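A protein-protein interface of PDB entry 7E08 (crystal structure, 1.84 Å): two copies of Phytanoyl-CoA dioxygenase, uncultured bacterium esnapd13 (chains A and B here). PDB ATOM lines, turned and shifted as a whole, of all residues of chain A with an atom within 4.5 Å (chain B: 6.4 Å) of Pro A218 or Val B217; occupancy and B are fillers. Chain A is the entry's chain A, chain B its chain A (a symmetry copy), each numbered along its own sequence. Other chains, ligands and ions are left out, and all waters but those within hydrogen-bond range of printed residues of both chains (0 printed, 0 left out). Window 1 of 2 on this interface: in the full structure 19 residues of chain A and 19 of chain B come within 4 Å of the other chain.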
ATOM      1  N   LYS A 107       1.469 -10.191 -10.357  1.00  0.00           N
ATOM      2  CA  LYS A 107       2.063  -8.928  -9.930  1.00  0.00           C
ATOM      3  C   LYS A 107       3.535  -9.195  -9.552  1.00  0.00           C
ATOM      4  O   LYS A 107       4.096 -10.259  -9.870  1.00  0.00           O
ATOM      5  CB  LYS A 107       1.216  -8.290  -8.807  1.00  0.00           C
ATOM      6  CG  LYS A 107       0.146  -7.342  -9.354  1.00  0.00           C
ATOM      7  CD  LYS A 107       0.420  -5.849  -9.136  1.00  0.00           C
ATOM      8  CE  LYS A 107       1.879  -5.394  -9.276  1.00  0.00           C
ATOM      9  NZ  LYS A 107       2.601  -5.118  -7.972  1.00  0.00           N
ATOM     10  N   GLY A 108       4.162  -8.177  -8.978  1.00  0.00           N
ATOM     11  CA  GLY A 108       5.423  -8.297  -8.317  1.00  0.00           C
ATOM     12  C   GLY A 108       6.461  -7.412  -8.890  1.00  0.00           C
ATOM     13  O   GLY A 108       6.387  -7.003 -10.065  1.00  0.00           O
ATOM     14  N   GLU A 109       7.467  -7.162  -8.050  1.00  0.00           N
ATOM     15  CA  GLU A 109       8.653  -6.376  -8.386  1.00  0.00           C
ATOM     16  C   GLU A 109       9.905  -7.254  -8.581  1.00  0.00           C
ATOM     17  O   GLU A 109      10.026  -8.341  -7.985  1.00  0.00           O
ATOM     18  CB  GLU A 109       8.922  -5.352  -7.266  1.00  0.00           C
ATOM     19  CG  GLU A 109       8.505  -3.912  -7.578  1.00  0.00           C
ATOM     20  CD  GLU A 109       7.097  -3.552  -7.144  1.00  0.00           C
ATOM     21  OE1 GLU A 109       6.899  -2.403  -6.671  1.00  0.00           O
ATOM     22  OE2 GLU A 109       6.185  -4.402  -7.287  1.00  0.00           O
ATOM     23  N   VAL A 110      10.834  -6.767  -9.421  1.00  0.00           N
ATOM     24  CA  VAL A 110      12.256  -7.177  -9.322  1.00  0.00           C
ATOM     25  C   VAL A 110      12.808  -6.499  -8.061  1.00  0.00           C
ATOM     26  O   VAL A 110      12.666  -5.279  -7.947  1.00  0.00           O
ATOM     27  CB  VAL A 110      13.151  -6.679 -10.501  1.00  0.00           C
ATOM     28  CG1 VAL A 110      14.536  -7.314 -10.376  1.00  0.00           C
ATOM     29  CG2 VAL A 110      12.517  -6.942 -11.870  1.00  0.00           C
ATOM     30  N   PHE A 144       7.985 -19.852 -10.260  1.00  0.00           N
ATOM     31  CA  PHE A 144       7.322 -18.846 -11.021  1.00  0.00           C
ATOM     32  C   PHE A 144       6.578 -17.806 -10.278  1.00  0.00           C
ATOM     33  O   PHE A 144       6.057 -16.903 -10.871  1.00  0.00           O
ATOM     34  CB  PHE A 144       6.359 -19.562 -12.049  1.00  0.00           C
ATOM     35  CG  PHE A 144       6.974 -20.725 -12.720  1.00  0.00           C
ATOM     36  CD1 PHE A 144       7.877 -20.502 -13.741  1.00  0.00           C
ATOM     37  CD2 PHE A 144       6.641 -21.995 -12.398  1.00  0.00           C
ATOM     38  CE1 PHE A 144       8.491 -21.558 -14.371  1.00  0.00           C
ATOM     39  CE2 PHE A 144       7.273 -23.073 -12.988  1.00  0.00           C
ATOM     40  CZ  PHE A 144       8.210 -22.827 -13.998  1.00  0.00           C
ATOM     41  N   GLY A 146       7.974 -15.658  -7.938  1.00  0.00           N
ATOM     42  CA  GLY A 146       8.936 -14.708  -7.364  1.00  0.00           C
ATOM     43  C   GLY A 146       9.647 -15.140  -6.066  1.00  0.00           C
ATOM     44  O   GLY A 146       9.618 -14.345  -5.116  1.00  0.00           O
ATOM     45  N   VAL A 217      12.240 -12.037  -8.365  1.00  0.00           N
ATOM     46  CA  VAL A 217      11.621 -11.412  -9.577  1.00  0.00           C
ATOM     47  C   VAL A 217      10.137 -11.399  -9.454  1.00  0.00           C
ATOM     48  O   VAL A 217       9.616 -11.877  -8.426  1.00  0.00           O
ATOM     49  CB  VAL A 217      11.956 -12.204 -10.828  1.00  0.00           C
ATOM     50  CG1 VAL A 217      13.462 -12.251 -11.051  1.00  0.00           C
ATOM     51  CG2 VAL A 217      11.393 -13.611 -10.761  1.00  0.00           C
ATOM     52  N   PRO A 218       9.412 -10.933 -10.517  1.00  0.00           N
ATOM     53  CA  PRO A 218       7.941 -11.002 -10.448  1.00  0.00           C
ATOM     54  C   PRO A 218       7.284 -12.314 -10.505  1.00  0.00           C
ATOM     55  O   PRO A 218       7.877 -13.326 -10.961  1.00  0.00           O
ATOM     56  CB  PRO A 218       7.471 -10.041 -11.554  1.00  0.00           C
ATOM     57  CG  PRO A 218       8.605  -9.067 -11.693  1.00  0.00           C
ATOM     58  CD  PRO A 218       9.844  -9.920 -11.505  1.00  0.00           C
ATOM     59  N   ASN A 219       6.076 -12.356  -9.890  1.00  0.00           N
ATOM     60  CA  ASN A 219       5.172 -13.559  -9.906  1.00  0.00           C
ATOM     61  C   ASN A 219       4.377 -13.531 -11.228  1.00  0.00           C
ATOM     62  O   ASN A 219       3.477 -12.686 -11.408  1.00  0.00           O
ATOM     63  CB  ASN A 219       4.196 -13.469  -8.745  1.00  0.00           C
ATOM     64  CG  ASN A 219       3.259 -14.628  -8.622  1.00  0.00           C
ATOM     65  OD1 ASN A 219       3.100 -15.523  -9.515  1.00  0.00           O
ATOM     66  ND2 ASN A 219       2.561 -14.650  -7.442  1.00  0.00           N
ATOM     67  N   ILE A 220       4.692 -14.466 -12.130  1.00  0.00           N
ATOM     68  CA  ILE A 220       3.952 -14.561 -13.431  1.00  0.00           C
ATOM     69  C   ILE A 220       2.942 -15.703 -13.336  1.00  0.00           C
ATOM     70  O   ILE A 220       2.317 -16.143 -14.355  1.00  0.00           O
ATOM     71  CB  ILE A 220       4.931 -14.745 -14.639  1.00  0.00           C
ATOM     72  CG1 ILE A 220       5.897 -15.920 -14.381  1.00  0.00           C
ATOM     73  CG2 ILE A 220       5.633 -13.417 -14.922  1.00  0.00           C
ATOM     74  CD1 ILE A 220       6.405 -16.659 -15.613  1.00  0.00           C
ATOM     75  N   LYS B 103      18.205 -10.574 -23.519  1.00  0.00           N
ATOM     76  CA  LYS B 103      17.964 -10.065 -22.175  1.00  0.00           C
ATOM     77  C   LYS B 103      19.250 -10.010 -21.529  1.00  0.00           C
ATOM     78  O   LYS B 103      19.788 -11.044 -21.173  1.00  0.00           O
ATOM     79  CB  LYS B 103      17.074 -11.014 -21.370  1.00  0.00           C
ATOM     80  CG  LYS B 103      15.614 -10.883 -21.681  1.00  0.00           C
ATOM     81  CD  LYS B 103      14.804 -11.707 -20.658  1.00  0.00           C
ATOM     82  CE  LYS B 103      13.364 -11.780 -21.117  1.00  0.00           C
ATOM     83  NZ  LYS B 103      12.686 -12.766 -20.290  1.00  0.00           N
ATOM     84  N   LYS B 107      19.110  -7.039 -16.561  1.00  0.00           N
ATOM     85  CA  LYS B 107      18.064  -6.289 -17.251  1.00  0.00           C
ATOM     86  C   LYS B 107      16.865  -7.236 -17.471  1.00  0.00           C
ATOM     87  O   LYS B 107      16.788  -8.322 -16.871  1.00  0.00           O
ATOM     88  CB  LYS B 107      18.625  -5.651 -18.540  1.00  0.00           C
ATOM     89  CG  LYS B 107      19.164  -4.238 -18.302  1.00  0.00           C
ATOM     90  CD  LYS B 107      18.300  -3.104 -18.864  1.00  0.00           C
ATOM     91  CE  LYS B 107      16.779  -3.286 -18.760  1.00  0.00           C
ATOM     92  NZ  LYS B 107      16.081  -3.669 -20.050  1.00  0.00           N
ATOM     93  N   GLY B 108      15.900  -6.751 -18.241  1.00  0.00           N
ATOM     94  CA  GLY B 108      14.845  -7.548 -18.782  1.00  0.00           C
ATOM     95  C   GLY B 108      13.502  -7.072 -18.387  1.00  0.00           C
ATOM     96  O   GLY B 108      13.332  -6.395 -17.354  1.00  0.00           O
ATOM     97  N   GLU B 109      12.532  -7.482 -19.206  1.00  0.00           N
ATOM     98  CA  GLU B 109      11.108  -7.213 -19.008  1.00  0.00           C
ATOM     99  C   GLU B 109      10.333  -8.459 -18.535  1.00  0.00           C
ATOM    100  O   GLU B 109      10.714  -9.606 -18.839  1.00  0.00           O
ATOM    101  CB  GLU B 109      10.496  -6.706 -20.328  1.00  0.00           C
ATOM    102  CG  GLU B 109      10.250  -5.197 -20.402  1.00  0.00           C
ATOM    103  CD  GLU B 109      11.397  -4.396 -20.987  1.00  0.00           C
ATOM    104  OE1 GLU B 109      11.118  -3.425 -21.737  1.00  0.00           O
ATOM    105  OE2 GLU B 109      12.573  -4.720 -20.691  1.00  0.00           O
ATOM    106  N   VAL B 110       9.241  -8.220 -17.790  1.00  0.00           N
ATOM    107  CA  VAL B 110       8.132  -9.200 -17.707  1.00  0.00           C
ATOM    108  C   VAL B 110       7.416  -9.150 -19.064  1.00  0.00           C
ATOM    109  O   VAL B 110       7.037  -8.052 -19.481  1.00  0.00           O
ATOM    110  CB  VAL B 110       7.047  -8.853 -16.639  1.00  0.00           C
ATOM    111  CG1 VAL B 110       6.067 -10.021 -16.528  1.00  0.00           C
ATOM    112  CG2 VAL B 110       7.657  -8.480 -15.284  1.00  0.00           C
ATOM    113  N   TRP B 111       7.295 -10.308 -19.742  1.00  0.00           N
ATOM    114  CA  TRP B 111       6.499 -10.433 -21.013  1.00  0.00           C
ATOM    115  C   TRP B 111       5.195 -11.134 -20.791  1.00  0.00           C
ATOM    116  O   TRP B 111       5.187 -12.367 -20.373  1.00  0.00           O
ATOM    117  CB  TRP B 111       7.168 -11.263 -22.072  1.00  0.00           C
ATOM    118  CG  TRP B 111       8.289 -10.629 -22.688  1.00  0.00           C
ATOM    119  CD1 TRP B 111       9.443 -10.234 -22.071  1.00  0.00           C
ATOM    120  CD2 TRP B 111       8.456 -10.365 -24.080  1.00  0.00           C
ATOM    121  NE1 TRP B 111      10.327  -9.731 -23.000  1.00  0.00           N
ATOM    122  CE2 TRP B 111       9.742  -9.789 -24.242  1.00  0.00           C
ATOM    123  CE3 TRP B 111       7.634 -10.520 -25.203  1.00  0.00           C
ATOM    124  CZ2 TRP B 111      10.234  -9.384 -25.487  1.00  0.00           C
ATOM    125  CZ3 TRP B 111       8.118 -10.102 -26.446  1.00  0.00           C
ATOM    126  CH2 TRP B 111       9.418  -9.550 -26.575  1.00  0.00           C
ATOM    127  N   GLU B 143      17.303 -20.857 -14.727  1.00  0.00           N
ATOM    128  CA  GLU B 143      16.137 -20.387 -14.004  1.00  0.00           C
ATOM    129  C   GLU B 143      16.090 -18.902 -13.836  1.00  0.00           C
ATOM    130  O   GLU B 143      14.989 -18.305 -13.685  1.00  0.00           O
ATOM    131  CB  GLU B 143      16.208 -21.159 -12.629  1.00  0.00           C
ATOM    132  CG  GLU B 143      15.032 -20.926 -11.739  1.00  0.00           C
ATOM    133  CD  GLU B 143      15.060 -21.732 -10.445  1.00  0.00           C
ATOM    134  OE1 GLU B 143      15.834 -22.672 -10.203  1.00  0.00           O
ATOM    135  OE2 GLU B 143      14.185 -21.356  -9.666  1.00  0.00           O
ATOM    136  N   PHE B 144      17.283 -18.243 -13.930  1.00  0.00           N
ATOM    137  CA  PHE B 144      17.418 -16.898 -13.476  1.00  0.00           C
ATOM    138  C   PHE B 144      17.695 -15.859 -14.491  1.00  0.00           C
ATOM    139  O   PHE B 144      17.754 -14.705 -14.166  1.00  0.00           O
ATOM    140  CB  PHE B 144      18.535 -16.866 -12.358  1.00  0.00           C
ATOM    141  CG  PHE B 144      18.431 -17.977 -11.390  1.00  0.00           C
ATOM    142  CD1 PHE B 144      17.463 -17.912 -10.406  1.00  0.00           C
ATOM    143  CD2 PHE B 144      19.285 -19.024 -11.409  1.00  0.00           C
ATOM    144  CE1 PHE B 144      17.316 -18.939  -9.504  1.00  0.00           C
ATOM    145  CE2 PHE B 144      19.133 -20.088 -10.539  1.00  0.00           C
ATOM    146  CZ  PHE B 144      18.125 -20.020  -9.569  1.00  0.00           C
ATOM    147  N   ASN B 145      17.773 -16.199 -15.795  1.00  0.00           N
ATOM    148  CA  ASN B 145      17.974 -15.179 -16.790  1.00  0.00           C
ATOM    149  C   ASN B 145      16.836 -15.014 -17.751  1.00  0.00           C
ATOM    150  O   ASN B 145      17.017 -14.721 -18.953  1.00  0.00           O
ATOM    151  CB  ASN B 145      19.282 -15.476 -17.616  1.00  0.00           C
ATOM    152  CG  ASN B 145      19.329 -16.833 -18.296  1.00  0.00           C
ATOM    153  OD1 ASN B 145      18.473 -17.713 -18.245  1.00  0.00           O
ATOM    154  ND2 ASN B 145      20.417 -16.961 -19.110  1.00  0.00           N
ATOM    155  N   GLY B 146      15.655 -15.144 -17.205  1.00  0.00           N
ATOM    156  CA  GLY B 146      14.416 -14.860 -17.940  1.00  0.00           C
ATOM    157  C   GLY B 146      14.026 -15.854 -19.052  1.00  0.00           C
ATOM    158  O   GLY B 146      13.769 -15.380 -20.168  1.00  0.00           O
ATOM    159  N   PRO B 147      14.015 -17.130 -18.763  1.00  0.00           N
ATOM    160  CA  PRO B 147      13.733 -18.101 -19.775  1.00  0.00           C
ATOM    161  C   PRO B 147      12.352 -18.013 -20.247  1.00  0.00           C
ATOM    162  O   PRO B 147      11.431 -17.643 -19.529  1.00  0.00           O
ATOM    163  CB  PRO B 147      14.001 -19.415 -19.094  1.00  0.00           C
ATOM    164  CG  PRO B 147      13.569 -19.174 -17.604  1.00  0.00           C
ATOM    165  CD  PRO B 147      14.152 -17.785 -17.420  1.00  0.00           C
ATOM    166  N   THR B 149       8.851 -19.254 -20.766  1.00  0.00           N
ATOM    167  CA  THR B 149       8.097 -20.059 -19.818  1.00  0.00           C
ATOM    168  C   THR B 149       6.732 -20.402 -20.490  1.00  0.00           C
ATOM    169  O   THR B 149       6.132 -19.564 -21.025  1.00  0.00           O
ATOM    170  CB  THR B 149       7.905 -19.291 -18.453  1.00  0.00           C
ATOM    171  OG1 THR B 149       9.207 -19.039 -17.916  1.00  0.00           O
ATOM    172  CG2 THR B 149       7.108 -20.121 -17.447  1.00  0.00           C
ATOM    173  N   SER B 215       5.531 -16.854 -21.776  1.00  0.00           N
ATOM    174  CA  SER B 215       5.793 -15.656 -20.988  1.00  0.00           C
ATOM    175  C   SER B 215       7.272 -15.755 -20.504  1.00  0.00           C
ATOM    176  O   SER B 215       7.869 -16.813 -20.535  1.00  0.00           O
ATOM    177  CB  SER B 215       4.938 -15.745 -19.706  1.00  0.00           C
ATOM    178  OG  SER B 215       5.090 -14.605 -18.871  1.00  0.00           O
ATOM    179  N   SER B 216       7.812 -14.683 -19.992  1.00  0.00           N
ATOM    180  CA  SER B 216       9.140 -14.748 -19.377  1.00  0.00           C
ATOM    181  C   SER B 216       9.316 -13.584 -18.404  1.00  0.00           C
ATOM    182  O   SER B 216       8.633 -12.611 -18.571  1.00  0.00           O
ATOM    183  CB  SER B 216      10.163 -14.691 -20.503  1.00  0.00           C
ATOM    184  OG  SER B 216      10.097 -13.453 -21.158  1.00  0.00           O
ATOM    185  N   VAL B 217      10.246 -13.673 -17.444  1.00  0.00           N
ATOM    186  CA  VAL B 217      10.476 -12.569 -16.457  1.00  0.00           C
ATOM    187  C   VAL B 217      11.821 -11.963 -16.662  1.00  0.00           C
ATOM    188  O   VAL B 217      12.550 -12.413 -17.569  1.00  0.00           O
ATOM    189  CB  VAL B 217      10.437 -13.096 -15.035  1.00  0.00           C
ATOM    190  CG1 VAL B 217       9.081 -13.715 -14.724  1.00  0.00           C
ATOM    191  CG2 VAL B 217      11.543 -14.104 -14.786  1.00  0.00           C
ATOM    192  N   PRO B 218      12.223 -10.991 -15.787  1.00  0.00           N
ATOM    193  CA  PRO B 218      13.586 -10.448 -15.917  1.00  0.00           C
ATOM    194  C   PRO B 218      14.731 -11.304 -15.577  1.00  0.00           C
ATOM    195  O   PRO B 218      14.596 -12.326 -14.855  1.00  0.00           O
ATOM    196  CB  PRO B 218      13.547  -9.140 -15.109  1.00  0.00           C
ATOM    197  CG  PRO B 218      12.103  -8.733 -15.150  1.00  0.00           C
ATOM    198  CD  PRO B 218      11.350 -10.046 -15.055  1.00  0.00           C
ATOM    199  N   ASN B 219      15.877 -10.983 -16.229  1.00  0.00           N
ATOM    200  CA  ASN B 219      17.200 -11.648 -15.968  1.00  0.00           C
ATOM    201  C   ASN B 219      17.836 -10.966 -14.740  1.00  0.00           C
ATOM    202  O   ASN B 219      18.285  -9.805 -14.821  1.00  0.00           O
ATOM    203  CB  ASN B 219      18.110 -11.444 -17.168  1.00  0.00           C
ATOM    204  CG  ASN B 219      19.453 -12.092 -17.054  1.00  0.00           C
ATOM    205  OD1 ASN B 219      19.924 -12.588 -15.979  1.00  0.00           O
ATOM    206  ND2 ASN B 219      20.159 -12.106 -18.230  1.00  0.00           N
ATOM    207  N   ARG B 225      20.918 -13.340 -21.779  1.00  0.00           N
ATOM    208  CA  ARG B 225      20.093 -14.425 -22.418  1.00  0.00           C
ATOM    209  C   ARG B 225      19.727 -14.105 -23.881  1.00  0.00           C
ATOM    210  O   ARG B 225      18.632 -13.644 -24.234  1.00  0.00           O
ATOM    211  CB  ARG B 225      18.837 -14.719 -21.614  1.00  0.00           C
ATOM    212  CG  ARG B 225      18.094 -15.972 -22.046  1.00  0.00           C
ATOM    213  CD  ARG B 225      16.633 -15.631 -22.143  1.00  0.00           C
ATOM    214  NE  ARG B 225      16.330 -14.735 -23.211  1.00  0.00           N
ATOM    215  CZ  ARG B 225      15.129 -14.415 -23.617  1.00  0.00           C
ATOM    216  NH1 ARG B 225      14.041 -14.860 -22.989  1.00  0.00           N
ATOM    217  NH2 ARG B 225      14.994 -13.664 -24.681  1.00  0.00           N
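N of Ile A220 sits at hydrogen-bond distance from O of Phe A144 (3.1 Å).
NZ of Lys B103 lies within hydrogen-bond range of O of Val B217 (2.7 Å).
O of Pro B147 lies within hydrogen-bond range of OG1 of Thr B149.
N of Thr B149 is in hydrogen-bond range of O of Ser B215 (2.6 Å).
CG of Pro B218 touches CG2 of Val A110, at 3.8 Å.
Thr B149 touches Phe A144.
Val A217 touches Pro B218 (CG1 to O, 3.97 Å).
Pro A218 touches Val B110 (CG to CG2, 3.8 Å).
Pro A218 touches Val B217 (O to CG1, 3.97 Å).
Pro A218 touches Pro B218 (CD to CD, 3.9 Å).
CG1 of Val B110 touches CG2 of Ile A220, at 3.8 Å.
Thr B149 touches Ile A220 (CG2 to CD1, 3.98 Å).
Ile A220 touches Val B217.
Of the printed residues of chain B, Val A110 touches Pro B218.
Of chain B, only Val B110, Val B217 and Pro B218 come within 4 Å of Pro A218.
Of the printed residues of chain B, Ile A220 touches Val B110, Thr B149 and Val B217.
Val B217 touches two residues of chain A.
The nearest printed residue of chain B that does not touch Pro A218 is Glu B109 (7.1 Å).
The nearest residue of chain A that does not touch Val B217 is Val A217 (4.1 Å).
The nearest printed residue of chain A that does not touch Pro B218 is Ile A220 (6.6 Å).
Along chain B the printed residues that touch a printed residue of chain A span positions 110 to 218.
Hydrophobic or aromatic side chains of chain A that line the printed part of chain B: Val A110, Phe A144, Val A217, Pro A218 and Ile A220.
Among the printed residues, 9 pairs touch across the chains.
Among the printed residues, no Asp or Glu carboxylate lies within 4 Å of a Lys or Arg side-chain nitrogen of the other chain.
Val A110 touches Pro B218, and with the chains exchanged Pro A218 touches Val B110.
Val A217 touches Pro B218, and with the chains exchanged Pro A218 touches Val B217.
Pro B218 touches its own counterpart, Pro A218.
Of the 9 pairs that touch across the chains among the printed residues, 5 have their exchanged pair printed and touching as well.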
